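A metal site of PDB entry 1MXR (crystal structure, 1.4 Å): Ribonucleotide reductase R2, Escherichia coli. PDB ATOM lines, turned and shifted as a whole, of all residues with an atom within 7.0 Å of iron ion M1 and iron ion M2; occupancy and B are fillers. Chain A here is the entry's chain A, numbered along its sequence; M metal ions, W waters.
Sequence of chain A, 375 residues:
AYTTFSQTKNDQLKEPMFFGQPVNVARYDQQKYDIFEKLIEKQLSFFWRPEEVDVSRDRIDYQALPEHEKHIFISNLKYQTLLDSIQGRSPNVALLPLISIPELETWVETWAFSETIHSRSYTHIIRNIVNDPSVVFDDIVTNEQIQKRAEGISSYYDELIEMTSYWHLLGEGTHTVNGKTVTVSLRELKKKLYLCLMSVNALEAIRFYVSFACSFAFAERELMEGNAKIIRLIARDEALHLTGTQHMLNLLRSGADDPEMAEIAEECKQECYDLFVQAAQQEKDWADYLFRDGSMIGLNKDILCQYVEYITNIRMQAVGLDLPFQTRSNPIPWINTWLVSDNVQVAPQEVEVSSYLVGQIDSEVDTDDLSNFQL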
ATOM      1  N   GLN A  80      19.643 -14.982  -1.446  1.00  0.00           N
ATOM      2  CA  GLN A  80      20.806 -15.854  -1.688  1.00  0.00           C
ATOM      3  C   GLN A  80      22.065 -14.996  -1.695  1.00  0.00           C
ATOM      4  O   GLN A  80      23.096 -15.409  -1.120  1.00  0.00           O
ATOM      5  CB  GLN A  80      20.666 -16.566  -3.054  1.00  0.00           C
ATOM      6  CG  GLN A  80      19.481 -17.568  -3.072  1.00  0.00           C
ATOM      7  CD  GLN A  80      19.167 -18.163  -4.462  1.00  0.00           C
ATOM      8  OE1 GLN A  80      19.307 -17.507  -5.489  1.00  0.00           O
ATOM      9  NE2 GLN A  80      18.739 -19.435  -4.479  1.00  0.00           N
ATOM     10  N   LEU A  83      23.012 -14.023   1.888  1.00  0.00           N
ATOM     11  CA  LEU A  83      23.597 -15.096   2.691  1.00  0.00           C
ATOM     12  C   LEU A  83      25.002 -15.428   2.264  1.00  0.00           C
ATOM     13  O   LEU A  83      25.888 -15.657   3.136  1.00  0.00           O
ATOM     14  CB  LEU A  83      22.734 -16.358   2.617  1.00  0.00           C
ATOM     15  CG  LEU A  83      21.356 -16.349   3.273  1.00  0.00           C
ATOM     16  CD1 LEU A  83      20.770 -17.731   3.243  1.00  0.00           C
ATOM     17  CD2 LEU A  83      21.453 -15.905   4.715  1.00  0.00           C
ATOM     18  N   ASP A  84      25.281 -15.454   0.976  1.00  0.00           N
ATOM     19  CA  ASP A  84      26.635 -15.775   0.566  1.00  0.00           C
ATOM     20  C   ASP A  84      27.628 -14.631   0.647  1.00  0.00           C
ATOM     21  O   ASP A  84      28.843 -14.869   0.636  1.00  0.00           O
ATOM     22  CB  ASP A  84      26.677 -16.531  -0.753  1.00  0.00           C
ATOM     23  CG  ASP A  84      26.514 -18.037  -0.511  1.00  0.00           C
ATOM     24  OD1 ASP A  84      26.417 -18.485   0.699  1.00  0.00           O
ATOM     25  OD2 ASP A  84      26.442 -18.785  -1.478  1.00  0.00           O
ATOM     26  N   GLN A  87      28.582 -15.513   4.049  1.00  0.00           N
ATOM     27  CA  GLN A  87      29.350 -16.768   4.041  1.00  0.00           C
ATOM     28  C   GLN A  87      30.704 -16.659   3.363  1.00  0.00           C
ATOM     29  O   GLN A  87      31.607 -17.467   3.607  1.00  0.00           O
ATOM     30  CB  GLN A  87      28.516 -17.937   3.427  1.00  0.00           C
ATOM     31  CG  GLN A  87      27.361 -18.400   4.303  1.00  0.00           C
ATOM     32  CD  GLN A  87      27.923 -19.037   5.558  1.00  0.00           C
ATOM     33  OE1 GLN A  87      28.328 -20.226   5.563  1.00  0.00           O
ATOM     34  NE2 GLN A  87      28.000 -18.267   6.609  1.00  0.00           N
ATOM     35  N   TRP A 111      36.146 -23.542   1.751  1.00  0.00           N
ATOM     36  CA  TRP A 111      34.720 -23.325   1.897  1.00  0.00           C
ATOM     37  C   TRP A 111      34.428 -21.844   1.674  1.00  0.00           C
ATOM     38  O   TRP A 111      33.579 -21.456   0.825  1.00  0.00           O
ATOM     39  CB  TRP A 111      34.366 -23.769   3.318  1.00  0.00           C
ATOM     40  CG  TRP A 111      32.991 -23.447   3.842  1.00  0.00           C
ATOM     41  CD1 TRP A 111      31.857 -23.110   3.151  1.00  0.00           C
ATOM     42  CD2 TRP A 111      32.618 -23.491   5.207  1.00  0.00           C
ATOM     43  NE1 TRP A 111      30.783 -22.951   4.028  1.00  0.00           N
ATOM     44  CE2 TRP A 111      31.250 -23.190   5.299  1.00  0.00           C
ATOM     45  CE3 TRP A 111      33.337 -23.794   6.386  1.00  0.00           C
ATOM     46  CZ2 TRP A 111      30.574 -23.175   6.527  1.00  0.00           C
ATOM     47  CZ3 TRP A 111      32.665 -23.771   7.603  1.00  0.00           C
ATOM     48  CH2 TRP A 111      31.304 -23.461   7.668  1.00  0.00           C
ATOM     49  N   SER A 114      34.908 -20.845  -1.905  1.00  0.00           N
ATOM     50  CA  SER A 114      33.839 -21.314  -2.784  1.00  0.00           C
ATOM     51  C   SER A 114      32.605 -20.419  -2.643  1.00  0.00           C
ATOM     52  O   SER A 114      31.843 -20.235  -3.623  1.00  0.00           O
ATOM     53  CB  SER A 114      33.514 -22.772  -2.502  1.00  0.00           C
ATOM     54  OG  SER A 114      32.738 -22.935  -1.336  1.00  0.00           O
ATOM     55  N   GLU A 115      32.373 -19.826  -1.483  1.00  0.00           N
ATOM     56  CA  GLU A 115      31.252 -18.902  -1.315  1.00  0.00           C
ATOM     57  C   GLU A 115      31.463 -17.623  -2.120  1.00  0.00           C
ATOM     58  O   GLU A 115      30.481 -17.022  -2.616  1.00  0.00           O
ATOM     59  CB  GLU A 115      31.074 -18.541   0.163  1.00  0.00           C
ATOM     60  CG  GLU A 115      30.813 -19.730   1.082  1.00  0.00           C
ATOM     61  CD  GLU A 115      29.478 -20.362   0.878  1.00  0.00           C
ATOM     62  OE1 GLU A 115      28.822 -20.071  -0.165  1.00  0.00           O
ATOM     63  OE2 GLU A 115      29.035 -21.139   1.743  1.00  0.00           O
ATOM     64  N   THR A 116      32.711 -17.147  -2.272  1.00  0.00           N
ATOM     65  CA  THR A 116      32.947 -15.950  -3.083  1.00  0.00           C
ATOM     66  C   THR A 116      32.639 -16.290  -4.537  1.00  0.00           C
ATOM     67  O   THR A 116      32.256 -15.374  -5.279  1.00  0.00           O
ATOM     68  CB  THR A 116      34.402 -15.365  -2.952  1.00  0.00           C
ATOM     69  OG1 THR A 116      35.377 -16.262  -3.518  1.00  0.00           O
ATOM     70  CG2 THR A 116      34.738 -15.114  -1.480  1.00  0.00           C
ATOM     71  N   HIS A 118      30.192 -18.311  -5.378  1.00  0.00           N
ATOM     72  CA  HIS A 118      28.718 -18.187  -5.423  1.00  0.00           C
ATOM     73  C   HIS A 118      28.333 -16.732  -5.572  1.00  0.00           C
ATOM     74  O   HIS A 118      27.451 -16.409  -6.399  1.00  0.00           O
ATOM     75  CB  HIS A 118      28.096 -18.782  -4.155  1.00  0.00           C
ATOM     76  CG  HIS A 118      28.370 -20.243  -4.045  1.00  0.00           C
ATOM     77  ND1 HIS A 118      27.948 -21.026  -2.991  1.00  0.00           N
ATOM     78  CD2 HIS A 118      29.056 -21.062  -4.868  1.00  0.00           C
ATOM     79  CE1 HIS A 118      28.355 -22.277  -3.181  1.00  0.00           C
ATOM     80  NE2 HIS A 118      29.040 -22.320  -4.316  1.00  0.00           N
ATOM     81  N   SER A 119      28.926 -15.829  -4.797  1.00  0.00           N
ATOM     82  CA  SER A 119      28.620 -14.395  -4.912  1.00  0.00           C
ATOM     83  C   SER A 119      28.884 -13.897  -6.308  1.00  0.00           C
ATOM     84  O   SER A 119      28.087 -13.151  -6.856  1.00  0.00           O
ATOM     85  CB  SER A 119      29.453 -13.592  -3.917  1.00  0.00           C
ATOM     86  OG  SER A 119      29.109 -13.997  -2.592  1.00  0.00           O
ATOM     87  N   TYR A 122      26.018 -14.796  -8.558  1.00  0.00           N
ATOM     88  CA  TYR A 122      24.821 -13.966  -8.414  1.00  0.00           C
ATOM     89  C   TYR A 122      25.033 -12.645  -9.159  1.00  0.00           C
ATOM     90  O   TYR A 122      24.090 -12.127  -9.788  1.00  0.00           O
ATOM     91  CB  TYR A 122      24.495 -13.706  -6.932  1.00  0.00           C
ATOM     92  CG  TYR A 122      24.319 -14.949  -6.132  1.00  0.00           C
ATOM     93  CD1 TYR A 122      23.548 -16.014  -6.588  1.00  0.00           C
ATOM     94  CD2 TYR A 122      24.950 -15.068  -4.875  1.00  0.00           C
ATOM     95  CE1 TYR A 122      23.414 -17.191  -5.815  1.00  0.00           C
ATOM     96  CE2 TYR A 122      24.807 -16.174  -4.136  1.00  0.00           C
ATOM     97  CZ  TYR A 122      24.062 -17.249  -4.588  1.00  0.00           C
ATOM     98  OH  TYR A 122      24.009 -18.381  -3.797  1.00  0.00           O
ATOM     99  N   LEU A 203      21.821 -22.490   8.426  1.00  0.00           N
ATOM    100  CA  LEU A 203      21.889 -21.581   7.296  1.00  0.00           C
ATOM    101  C   LEU A 203      22.096 -22.298   5.976  1.00  0.00           C
ATOM    102  O   LEU A 203      21.317 -22.118   5.005  1.00  0.00           O
ATOM    103  CB  LEU A 203      23.051 -20.594   7.526  1.00  0.00           C
ATOM    104  CG  LEU A 203      23.285 -19.410   6.574  1.00  0.00           C
ATOM    105  CD1 LEU A 203      24.275 -18.412   7.202  1.00  0.00           C
ATOM    106  CD2 LEU A 203      23.843 -19.877   5.190  1.00  0.00           C
ATOM    107  N   GLU A 204      23.126 -23.127   5.910  1.00  0.00           N
ATOM    108  CA  GLU A 204      23.384 -23.813   4.633  1.00  0.00           C
ATOM    109  C   GLU A 204      22.487 -25.000   4.372  1.00  0.00           C
ATOM    110  O   GLU A 204      22.112 -25.236   3.222  1.00  0.00           O
ATOM    111  CB  GLU A 204      24.835 -24.228   4.588  1.00  0.00           C
ATOM    112  CG  GLU A 204      25.754 -23.012   4.621  1.00  0.00           C
ATOM    113  CD  GLU A 204      27.223 -23.371   4.458  1.00  0.00           C
ATOM    114  OE1 GLU A 204      27.735 -24.199   5.261  1.00  0.00           O
ATOM    115  OE2 GLU A 204      27.860 -22.822   3.504  1.00  0.00           O
ATOM    116  N   PHE A 208      19.283 -22.156   2.727  1.00  0.00           N
ATOM    117  CA  PHE A 208      19.623 -22.161   1.304  1.00  0.00           C
ATOM    118  C   PHE A 208      18.811 -23.172   0.530  1.00  0.00           C
ATOM    119  O   PHE A 208      18.510 -22.932  -0.666  1.00  0.00           O
ATOM    120  CB  PHE A 208      21.120 -22.385   1.115  1.00  0.00           C
ATOM    121  CG  PHE A 208      21.854 -21.133   0.722  1.00  0.00           C
ATOM    122  CD1 PHE A 208      21.606 -20.565  -0.529  1.00  0.00           C
ATOM    123  CD2 PHE A 208      22.736 -20.492   1.595  1.00  0.00           C
ATOM    124  CE1 PHE A 208      22.232 -19.377  -0.909  1.00  0.00           C
ATOM    125  CE2 PHE A 208      23.373 -19.296   1.216  1.00  0.00           C
ATOM    126  CZ  PHE A 208      23.115 -18.736  -0.037  1.00  0.00           C
ATOM    127  N   PHE A 212      16.780 -22.731  -2.841  1.00  0.00           N
ATOM    128  CA  PHE A 212      17.022 -23.508  -4.054  1.00  0.00           C
ATOM    129  C   PHE A 212      15.678 -23.964  -4.619  1.00  0.00           C
ATOM    130  O   PHE A 212      15.471 -23.956  -5.835  1.00  0.00           O
ATOM    131  CB  PHE A 212      17.888 -24.756  -3.786  1.00  0.00           C
ATOM    132  CG  PHE A 212      19.287 -24.447  -3.301  1.00  0.00           C
ATOM    133  CD1 PHE A 212      19.924 -23.245  -3.592  1.00  0.00           C
ATOM    134  CD2 PHE A 212      19.964 -25.400  -2.539  1.00  0.00           C
ATOM    135  CE1 PHE A 212      21.238 -22.989  -3.115  1.00  0.00           C
ATOM    136  CE2 PHE A 212      21.269 -25.131  -2.074  1.00  0.00           C
ATOM    137  CZ  PHE A 212      21.862 -23.945  -2.366  1.00  0.00           C
ATOM    138  N   ILE A 234      25.834 -24.455  -7.355  1.00  0.00           N
ATOM    139  CA  ILE A 234      25.859 -23.938  -5.978  1.00  0.00           C
ATOM    140  C   ILE A 234      25.357 -24.995  -4.987  1.00  0.00           C
ATOM    141  O   ILE A 234      25.993 -25.226  -3.915  1.00  0.00           O
ATOM    142  CB  ILE A 234      25.036 -22.631  -5.859  1.00  0.00           C
ATOM    143  CG1 ILE A 234      25.781 -21.502  -6.581  1.00  0.00           C
ATOM    144  CG2 ILE A 234      24.789 -22.284  -4.344  1.00  0.00           C
ATOM    145  CD1 ILE A 234      25.013 -20.182  -6.571  1.00  0.00           C
ATOM    146  N   ASP A 237      27.862 -27.610  -4.207  1.00  0.00           N
ATOM    147  CA  ASP A 237      28.860 -27.113  -3.214  1.00  0.00           C
ATOM    148  C   ASP A 237      28.227 -27.049  -1.821  1.00  0.00           C
ATOM    149  O   ASP A 237      28.868 -27.451  -0.849  1.00  0.00           O
ATOM    150  CB  ASP A 237      29.310 -25.694  -3.580  1.00  0.00           C
ATOM    151  CG  ASP A 237      30.149 -25.626  -4.858  1.00  0.00           C
ATOM    152  OD1 ASP A 237      30.736 -26.659  -5.231  1.00  0.00           O
ATOM    153  OD2 ASP A 237      30.196 -24.513  -5.406  1.00  0.00           O
ATOM    154  N   GLU A 238      27.004 -26.547  -1.724  1.00  0.00           N
ATOM    155  CA  GLU A 238      26.350 -26.428  -0.437  1.00  0.00           C
ATOM    156  C   GLU A 238      26.238 -27.758   0.274  1.00  0.00           C
ATOM    157  O   GLU A 238      26.332 -27.838   1.531  1.00  0.00           O
ATOM    158  CB  GLU A 238      24.945 -25.849  -0.612  1.00  0.00           C
ATOM    159  CG  GLU A 238      24.366 -25.326   0.668  1.00  0.00           C
ATOM    160  CD  GLU A 238      25.010 -24.011   1.088  1.00  0.00           C
ATOM    161  OE1 GLU A 238      24.415 -22.963   0.865  1.00  0.00           O
ATOM    162  OE2 GLU A 238      26.130 -24.003   1.645  1.00  0.00           O
ATOM    163  N   ALA A 239      26.066 -28.831  -0.487  1.00  0.00           N
ATOM    164  CA  ALA A 239      25.964 -30.158   0.139  1.00  0.00           C
ATOM    165  C   ALA A 239      27.292 -30.472   0.856  1.00  0.00           C
ATOM    166  O   ALA A 239      27.303 -31.091   1.922  1.00  0.00           O
ATOM    167  CB  ALA A 239      25.639 -31.235  -0.934  1.00  0.00           C
ATOM    168  N   HIS A 241      29.333 -28.147   2.070  1.00  0.00           N
ATOM    169  CA  HIS A 241      29.425 -27.217   3.211  1.00  0.00           C
ATOM    170  C   HIS A 241      28.660 -27.723   4.417  1.00  0.00           C
ATOM    171  O   HIS A 241      29.187 -27.738   5.518  1.00  0.00           O
ATOM    172  CB  HIS A 241      28.939 -25.822   2.848  1.00  0.00           C
ATOM    173  CG  HIS A 241      29.651 -25.247   1.655  1.00  0.00           C
ATOM    174  ND1 HIS A 241      29.268 -24.066   1.058  1.00  0.00           N
ATOM    175  CD2 HIS A 241      30.740 -25.680   0.984  1.00  0.00           C
ATOM    176  CE1 HIS A 241      30.106 -23.794   0.073  1.00  0.00           C
ATOM    177  NE2 HIS A 241      30.999 -24.757   0.001  1.00  0.00           N
ATOM    178  N   LEU A 242      27.420 -28.164   4.228  1.00  0.00           N
ATOM    179  CA  LEU A 242      26.655 -28.670   5.370  1.00  0.00           C
ATOM    180  C   LEU A 242      27.214 -30.016   5.843  1.00  0.00           C
ATOM    181  O   LEU A 242      27.128 -30.368   7.047  1.00  0.00           O
ATOM    182  CB  LEU A 242      25.154 -28.740   4.980  1.00  0.00           C
ATOM    183  CG  LEU A 242      24.756 -29.854   3.972  1.00  0.00           C
ATOM    184  CD1 LEU A 242      24.384 -31.184   4.648  1.00  0.00           C
ATOM    185  CD2 LEU A 242      23.563 -29.360   3.099  1.00  0.00           C
HETATM  186 FE    FE M   1      27.651 -22.631   1.572  1.00  0.00          FE
HETATM  187 FE    FE M   2      27.104 -20.615  -1.081  1.00  0.00          FE
HETATM  188  O   HOH W   1      24.884 -21.181  -1.324  1.00  0.00           O
HETATM  189  O   HOH W   2      26.017 -21.046   1.916  1.00  0.00           O
HETATM  190  O   HOH W   3      27.293 -22.377  -0.313  1.00  0.00           O
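NE1 of Trp 111 sits close to OE2 of Glu 204 (3.0 Å).
The side-chain carboxylate (OE2) of Glu 204 lies close to the side-chain amide oxygen (OE1) of Gln 87 (3.3 Å).
OD2 of Asp 84 sits close to OH of Tyr 122 (3.4 Å).
O of Asp 84 lies within hydrogen-bond range of OG of Ser 119, 3.4 Å away.
The backbone carbonyl oxygen of Glu 115 lies within hydrogen-bond range of the side-chain hydroxyl of Ser 119, at 3.3 Å.
OD2 of Asp 237 sits at hydrogen-bond distance from NE2 of His 118 (2.7 Å).
The side-chain hydroxyl (OG) of Ser 114 sits at hydrogen-bond distance from a ring nitrogen (NE2) of His 241, at 2.9 Å.
The side-chain hydroxyl (OG) of Ser 114 sits at hydrogen-bond distance from the backbone carbonyl oxygen (O) of Trp 111 (2.8 Å).
Merely in contact with iron ion M1: Trp 111 (3.99 Å).
Five residues have an atom within 4 Å of iron ion M1: Trp 111, Glu 115, Glu 204, Glu 238 and His 241.
Within 4 Å of iron ion M2: Asp 84, Glu 115 and His 118.
The nearest printed residue that does not touch iron ion M2 is Glu 238 (4.1 Å).
Iron ion M1 is bound by water W3 (1.9 Å), OE2 of Glu 204 (2.0 Å), OE2 of Glu 115 (2.0 Å), OE2 of Glu 238 (2.0 Å), ND1 of His 241 (2.2 Å) and water W2 (2.3 Å).
Iron ion M2 is bound by water W3, the side-chain carboxylate of Asp 84, the side-chain carboxylate of Glu 115, a ring nitrogen (ND1) of His 118 and water W1.
Iron ion M2 has five donor atoms within binding distance.
Water W2 bridges OE1 of Glu 238 (2.7 Å) and OD1 of Asp 84 (2.9 Å).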
